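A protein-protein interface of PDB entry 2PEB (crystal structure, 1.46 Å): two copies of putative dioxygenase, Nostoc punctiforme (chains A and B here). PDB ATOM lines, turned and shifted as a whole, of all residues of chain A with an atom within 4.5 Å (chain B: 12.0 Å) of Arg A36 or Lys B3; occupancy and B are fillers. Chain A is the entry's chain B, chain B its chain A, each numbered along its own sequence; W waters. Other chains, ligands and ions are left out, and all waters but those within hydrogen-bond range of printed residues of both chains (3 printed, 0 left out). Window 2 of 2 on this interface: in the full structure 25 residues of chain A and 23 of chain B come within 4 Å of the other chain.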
ATOM      1  N   ARG A  28       9.628   6.720  10.515  1.00  0.00           N
ATOM      2  CA  ARG A  28      10.458   7.315   9.476  1.00  0.00           C
ATOM      3  C   ARG A  28      10.217   6.621   8.154  1.00  0.00           C
ATOM      4  O   ARG A  28      10.169   7.269   7.116  1.00  0.00           O
ATOM      5  CB  ARG A  28      11.949   7.300   9.859  1.00  0.00           C
ATOM      6  CG  ARG A  28      12.221   8.066  11.163  1.00  0.00           C
ATOM      7  CD  ARG A  28      13.711   8.339  11.420  1.00  0.00           C
ATOM      8  NE  ARG A  28      14.589   7.167  11.267  1.00  0.00           N
ATOM      9  CZ  ARG A  28      15.026   6.371  12.255  1.00  0.00           C
ATOM     10  NH1 ARG A  28      14.682   6.560  13.531  1.00  0.00           N
ATOM     11  NH2 ARG A  28      15.828   5.360  11.955  1.00  0.00           N
ATOM     12  N   GLU A  31       6.980   7.984   6.728  1.00  0.00           N
ATOM     13  CA  GLU A  31       7.146   9.293   6.133  1.00  0.00           C
ATOM     14  C   GLU A  31       7.812   9.176   4.774  1.00  0.00           C
ATOM     15  O   GLU A  31       7.418   9.869   3.830  1.00  0.00           O
ATOM     16  CB  GLU A  31       7.923  10.226   7.047  1.00  0.00           C
ATOM     17  CG  GLU A  31       8.067  11.692   6.566  1.00  0.00           C
ATOM     18  CD  GLU A  31       9.147  11.922   5.496  1.00  0.00           C
ATOM     19  OE1 GLU A  31      10.181  11.200   5.497  1.00  0.00           O
ATOM     20  OE2 GLU A  31       8.973  12.856   4.663  1.00  0.00           O
ATOM     21  N   GLY A  32       8.776   8.270   4.651  1.00  0.00           N
ATOM     22  CA  GLY A  32       9.424   8.039   3.395  1.00  0.00           C
ATOM     23  C   GLY A  32       8.442   7.601   2.322  1.00  0.00           C
ATOM     24  O   GLY A  32       8.495   8.061   1.185  1.00  0.00           O
ATOM     25  N   LEU A  33       7.577   6.662   2.676  1.00  0.00           N
ATOM     26  CA  LEU A  33       6.572   6.155   1.743  1.00  0.00           C
ATOM     27  C   LEU A  33       5.621   7.256   1.306  1.00  0.00           C
ATOM     28  O   LEU A  33       5.364   7.459   0.122  1.00  0.00           O
ATOM     29  CB  LEU A  33       5.767   5.052   2.416  1.00  0.00           C
ATOM     30  CG  LEU A  33       6.545   3.759   2.653  1.00  0.00           C
ATOM     31  CD1 LEU A  33       5.805   2.796   3.572  1.00  0.00           C
ATOM     32  CD2 LEU A  33       6.832   3.104   1.343  1.00  0.00           C
ATOM     33  N   GLY A  34       5.081   7.982   2.283  1.00  0.00           N
ATOM     34  CA  GLY A  34       4.099   8.999   1.998  1.00  0.00           C
ATOM     35  C   GLY A  34       4.662  10.166   1.207  1.00  0.00           C
ATOM     36  O   GLY A  34       3.913  10.836   0.510  1.00  0.00           O
ATOM     37  N   ALA A  35       5.978  10.408   1.312  1.00  0.00           N
ATOM     38  CA  ALA A  35       6.646  11.513   0.596  1.00  0.00           C
ATOM     39  C   ALA A  35       6.875  11.148  -0.861  1.00  0.00           C
ATOM     40  O   ALA A  35       6.948  12.022  -1.718  1.00  0.00           O
ATOM     41  CB  ALA A  35       8.024  11.787   1.232  1.00  0.00           C
ATOM     42  N   ARG A  36       7.037   9.856  -1.128  1.00  0.00           N
ATOM     43  CA  ARG A  36       7.591   9.375  -2.406  1.00  0.00           C
ATOM     44  C   ARG A  36       6.626   8.697  -3.369  1.00  0.00           C
ATOM     45  O   ARG A  36       6.800   8.783  -4.595  1.00  0.00           O
ATOM     46  CB  ARG A  36       8.698   8.394  -2.118  1.00  0.00           C
ATOM     47  CG  ARG A  36       9.960   9.032  -1.679  1.00  0.00           C
ATOM     48  CD  ARG A  36      11.007   7.959  -1.338  1.00  0.00           C
ATOM     49  NE  ARG A  36      12.249   8.616  -0.948  1.00  0.00           N
ATOM     50  CZ  ARG A  36      12.469   9.161   0.238  1.00  0.00           C
ATOM     51  NH1 ARG A  36      11.547   9.081   1.180  1.00  0.00           N
ATOM     52  NH2 ARG A  36      13.633   9.772   0.495  1.00  0.00           N
ATOM     53  N   PHE A  37       5.638   7.992  -2.841  1.00  0.00           N
ATOM     54  CA  PHE A  37       4.856   7.041  -3.647  1.00  0.00           C
ATOM     55  C   PHE A  37       3.377   7.355  -3.583  1.00  0.00           C
ATOM     56  O   PHE A  37       2.940   8.106  -2.723  1.00  0.00           O
ATOM     57  CB  PHE A  37       5.162   5.616  -3.238  1.00  0.00           C
ATOM     58  CG  PHE A  37       6.627   5.330  -3.260  1.00  0.00           C
ATOM     59  CD1 PHE A  37       7.348   5.425  -4.459  1.00  0.00           C
ATOM     60  CD2 PHE A  37       7.323   5.051  -2.080  1.00  0.00           C
ATOM     61  CE1 PHE A  37       8.739   5.177  -4.478  1.00  0.00           C
ATOM     62  CE2 PHE A  37       8.697   4.822  -2.090  1.00  0.00           C
ATOM     63  CZ  PHE A  37       9.400   4.883  -3.306  1.00  0.00           C
ATOM     64  N   TRP A  72      11.964   0.153  -2.925  1.00  0.00           N
ATOM     65  CA  TRP A  72      12.324   1.157  -1.935  1.00  0.00           C
ATOM     66  C   TRP A  72      12.374   0.548  -0.536  1.00  0.00           C
ATOM     67  O   TRP A  72      13.321   0.785   0.222  1.00  0.00           O
ATOM     68  CB  TRP A  72      11.361   2.344  -1.980  1.00  0.00           C
ATOM     69  CG  TRP A  72      11.885   3.483  -1.175  1.00  0.00           C
ATOM     70  CD1 TRP A  72      12.773   4.447  -1.574  1.00  0.00           C
ATOM     71  CD2 TRP A  72      11.554   3.791   0.194  1.00  0.00           C
ATOM     72  NE1 TRP A  72      13.032   5.308  -0.543  1.00  0.00           N
ATOM     73  CE2 TRP A  72      12.279   4.948   0.544  1.00  0.00           C
ATOM     74  CE3 TRP A  72      10.722   3.189   1.150  1.00  0.00           C
ATOM     75  CZ2 TRP A  72      12.203   5.508   1.821  1.00  0.00           C
ATOM     76  CZ3 TRP A  72      10.635   3.762   2.400  1.00  0.00           C
ATOM     77  CH2 TRP A  72      11.372   4.902   2.718  1.00  0.00           C
ATOM     78  N   ASN A  76      15.187   0.290   2.283  1.00  0.00           N
ATOM     79  CA  ASN A  76      15.046   1.345   3.295  1.00  0.00           C
ATOM     80  C   ASN A  76      14.230   0.956   4.503  1.00  0.00           C
ATOM     81  O   ASN A  76      13.902   1.810   5.308  1.00  0.00           O
ATOM     82  CB  ASN A  76      14.465   2.627   2.666  1.00  0.00           C
ATOM     83  CG  ASN A  76      15.447   3.328   1.756  1.00  0.00           C
ATOM     84  OD1 ASN A  76      16.388   3.957   2.221  1.00  0.00           O
ATOM     85  ND2 ASN A  76      15.252   3.217   0.470  1.00  0.00           N
ATOM     86  N   LYS B   3      18.200   8.388   2.651  1.00  0.00           N
ATOM     87  CA  LYS B   3      17.673   7.073   2.198  1.00  0.00           C
ATOM     88  C   LYS B   3      18.553   6.482   1.078  1.00  0.00           C
ATOM     89  O   LYS B   3      19.370   7.182   0.452  1.00  0.00           O
ATOM     90  CB  LYS B   3      16.209   7.209   1.727  1.00  0.00           C
ATOM     91  CG  LYS B   3      15.245   7.818   2.772  1.00  0.00           C
ATOM     92  CD  LYS B   3      15.005   6.905   3.985  1.00  0.00           C
ATOM     93  CE  LYS B   3      13.973   7.479   4.964  1.00  0.00           C
ATOM     94  NZ  LYS B   3      12.776   8.061   4.289  1.00  0.00           N
ATOM     95  N   GLU B   4      18.387   5.181   0.863  1.00  0.00           N
ATOM     96  CA  GLU B   4      19.010   4.465  -0.240  1.00  0.00           C
ATOM     97  C   GLU B   4      18.199   4.657  -1.520  1.00  0.00           C
ATOM     98  O   GLU B   4      16.953   4.484  -1.520  1.00  0.00           O
ATOM     99  CB  GLU B   4      19.051   2.977   0.083  1.00  0.00           C
ATOM    100  CG  GLU B   4      20.041   2.193  -0.772  1.00  0.00           C
ATOM    101  CD  GLU B   4      21.268   1.743  -0.001  1.00  0.00           C
ATOM    102  OE1 GLU B   4      21.098   1.206   1.118  1.00  0.00           O
ATOM    103  OE2 GLU B   4      22.391   1.910  -0.523  1.00  0.00           O
ATOM    104  N   ASP B   5      18.900   5.009  -2.603  1.00  0.00           N
ATOM    105  CA  ASP B   5      18.254   5.249  -3.904  1.00  0.00           C
ATOM    106  C   ASP B   5      18.100   3.938  -4.690  1.00  0.00           C
ATOM    107  O   ASP B   5      19.092   3.226  -4.959  1.00  0.00           O
ATOM    108  CB  ASP B   5      19.020   6.285  -4.736  1.00  0.00           C
ATOM    109  CG  ASP B   5      19.177   7.611  -4.020  1.00  0.00           C
ATOM    110  OD1 ASP B   5      18.552   7.815  -2.952  1.00  0.00           O
ATOM    111  OD2 ASP B   5      19.945   8.461  -4.532  1.00  0.00           O
ATOM    112  N   THR B   6      16.849   3.622  -5.039  1.00  0.00           N
ATOM    113  CA  THR B   6      16.541   2.402  -5.807  1.00  0.00           C
ATOM    114  C   THR B   6      17.055   2.500  -7.247  1.00  0.00           C
ATOM    115  O   THR B   6      17.021   1.523  -7.990  1.00  0.00           O
ATOM    116  CB  THR B   6      15.025   2.086  -5.812  1.00  0.00           C
ATOM    117  OG1 THR B   6      14.330   3.089  -6.565  1.00  0.00           O
ATOM    118  CG2 THR B   6      14.478   2.072  -4.402  1.00  0.00           C
ATOM    119  N   ILE B   7      17.536   3.677  -7.652  1.00  0.00           N
ATOM    120  CA  ILE B   7      18.304   3.775  -8.894  1.00  0.00           C
ATOM    121  C   ILE B   7      19.512   2.835  -8.787  1.00  0.00           C
ATOM    122  O   ILE B   7      19.933   2.227  -9.757  1.00  0.00           O
ATOM    123  CB  ILE B   7      18.808   5.205  -9.151  1.00  0.00           C
ATOM    124  CG1 ILE B   7      19.054   5.443 -10.650  1.00  0.00           C
ATOM    125  CG2 ILE B   7      20.076   5.464  -8.344  1.00  0.00           C
ATOM    126  CD1 ILE B   7      17.817   5.366 -11.539  1.00  0.00           C
ATOM    127  N   GLU B   8      20.031   2.679  -7.577  1.00  0.00           N
ATOM    128  CA  GLU B   8      21.166   1.842  -7.374  1.00  0.00           C
ATOM    129  C   GLU B   8      20.846   0.378  -7.648  1.00  0.00           C
ATOM    130  O   GLU B   8      21.757  -0.424  -7.582  1.00  0.00           O
ATOM    131  CB  GLU B   8      21.707   2.014  -5.952  1.00  0.00           C
ATOM    132  CG  GLU B   8      21.181   1.029  -4.919  1.00  0.00           C
ATOM    133  CD  GLU B   8      21.665   1.358  -3.527  1.00  0.00           C
ATOM    134  OE1 GLU B   8      21.980   2.546  -3.267  1.00  0.00           O
ATOM    135  OE2 GLU B   8      21.733   0.433  -2.694  1.00  0.00           O
ATOM    136  N   ILE B   9      19.585   0.031  -7.956  1.00  0.00           N
ATOM    137  CA  ILE B   9      19.202  -1.357  -8.305  1.00  0.00           C
ATOM    138  C   ILE B   9      19.305  -1.532  -9.802  1.00  0.00           C
ATOM    139  O   ILE B   9      18.534  -0.930 -10.554  1.00  0.00           O
ATOM    140  CB  ILE B   9      17.780  -1.756  -7.869  1.00  0.00           C
ATOM    141  CG1 ILE B   9      17.620  -1.671  -6.346  1.00  0.00           C
ATOM    142  CG2 ILE B   9      17.464  -3.181  -8.285  1.00  0.00           C
ATOM    143  CD1 ILE B   9      16.137  -1.918  -5.918  1.00  0.00           C
ATOM    144  N   THR B  88      22.925  -4.509  -6.662  1.00  0.00           N
ATOM    145  CA  THR B  88      23.325  -3.154  -6.417  1.00  0.00           C
ATOM    146  C   THR B  88      24.836  -3.027  -6.275  1.00  0.00           C
ATOM    147  O   THR B  88      25.347  -1.937  -5.986  1.00  0.00           O
ATOM    148  CB  THR B  88      22.712  -2.639  -5.105  1.00  0.00           C
ATOM    149  OG1 THR B  88      23.329  -3.324  -4.013  1.00  0.00           O
ATOM    150  CG2 THR B  88      21.203  -2.874  -5.084  1.00  0.00           C
ATOM    151  N   TYR B  98      18.705  -6.741   1.621  1.00  0.00           N
ATOM    152  CA  TYR B  98      17.872  -6.088   0.650  1.00  0.00           C
ATOM    153  C   TYR B  98      16.943  -7.060  -0.028  1.00  0.00           C
ATOM    154  O   TYR B  98      16.281  -6.663  -0.977  1.00  0.00           O
ATOM    155  CB  TYR B  98      18.694  -5.342  -0.432  1.00  0.00           C
ATOM    156  CG  TYR B  98      19.660  -4.303   0.050  1.00  0.00           C
ATOM    157  CD1 TYR B  98      19.406  -3.540   1.193  1.00  0.00           C
ATOM    158  CD2 TYR B  98      20.821  -4.056  -0.655  1.00  0.00           C
ATOM    159  CE1 TYR B  98      20.269  -2.561   1.595  1.00  0.00           C
ATOM    160  CE2 TYR B  98      21.697  -3.086  -0.259  1.00  0.00           C
ATOM    161  CZ  TYR B  98      21.427  -2.369   0.886  1.00  0.00           C
ATOM    162  OH  TYR B  98      22.305  -1.432   1.274  1.00  0.00           O
HETATM  163  O   HOH W   1      11.976  10.597   3.599  1.00  0.00           O
HETATM  164  O   HOH W   2      15.242   6.961  -1.581  1.00  0.00           O
HETATM  165  O   HOH W   3      11.755   9.557   6.721  1.00  0.00           O
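OE1 of Glu B4 sits at hydrogen-bond distance from OH of Tyr B98, 2.9 Å away.
The side-chain carboxylate of Glu B4 sits close to the side-chain carboxylate of Glu B8 (2.7 Å).
The guanidinium group (NH1) of Arg A36 lies within hydrogen-bond range of the backbone carbonyl oxygen (O) of Gly A32 (3.2 Å).
The backbone carbonyl oxygen (O) of Trp A72 lies within hydrogen-bond range of the side-chain amide nitrogen (ND2) of Asn A76, at 3.1 Å.
Arg A28 touches Lys B3.
Gly A32 touches Lys B3.
Lys B3 touches Trp A72.
Thr B6 touches Trp A72 (CG2 to CA, 3.4 Å).
OD1 of Asn A76 touches CB of Lys B3 (3.3 Å).
Of the 10 printed residues of chain A, 5 touch a printed residue of chain B.
Printed residues of chain A that touch a printed residue of chain B: Arg A28, Gly A32, Arg A36, Trp A72 and Asn A76.
Hydrophobic or aromatic side chains of chain A that line the printed part of chain B: Trp A72.
Along chain B the printed residues that touch a printed residue of chain A span positions 3 to 6.
Among the printed residues, no Asp or Glu carboxylate lies within 4 Å of a Lys or Arg side-chain nitrogen of the other chain.
Of the printed residues of chain B, Arg A28 touches Lys B3.
Glu A31 touches none of the printed residues of chain B.
Printed residues of chain B within 4 Å of Gly A32: Lys B3 (3.5 Å).
No residue of chain B comes within 4 Å of Gly A34.
Arg A36 touches one residue of chain B.
Phe A37 touches none of the printed residues of chain B.
Of the printed residues of chain B, Trp A72 touches Lys B3 (3.6 Å) and Thr B6 (3.4 Å).
Asn A76 touches just these residues of chain B: Lys B3 and Glu B4.
Of chain A, only Arg A28, Gly A32, Arg A36, Trp A72 and Asn A76 come within 4 Å of Lys B3.
Printed residues of chain A within 4 Å of Glu B4: Asn A76 (2.7 Å).
Of the printed residues of chain A, Thr B6 touches Trp A72 (3.4 Å).
Glu B8 touches none of the printed residues of chain A.
Thr B88 touches none of the printed residues of chain A.
The nearest residue of chain A that does not touch Lys B3 is Glu A31 (4.2 Å).
The nearest printed residue of chain A that does not touch Thr B6 is Asn A76 (5.1 Å).
NH1 of Arg A36 lies close to NZ of Lys B3, at 3.5 Å.
The side-chain amide oxygen (OD1) of Asn A76 sits at hydrogen-bond distance from the backbone NH (N) of Glu B4 (2.7 Å).
No position is printed for both chains.
Of the 7 pairs that touch across the chains among the printed residues, none has its exchanged pair printed and touching as well.
Water W3 lies within hydrogen-bond range of OE1 of Glu A31 (2.6 Å), O of Arg A28 (2.8 Å) and NZ of Lys B3 (3.0 Å).
Water W1 lies within hydrogen-bond range of the side-chain carboxylate of Glu A31, the side-chain amino group of Lys B3 and the guanidinium group of Arg A36.
Water W2 lies within hydrogen-bond range of NE1 of Trp A72 (2.9 Å), O of Glu B4 (3.0 Å) and NE of Arg A36 (3.5 Å).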
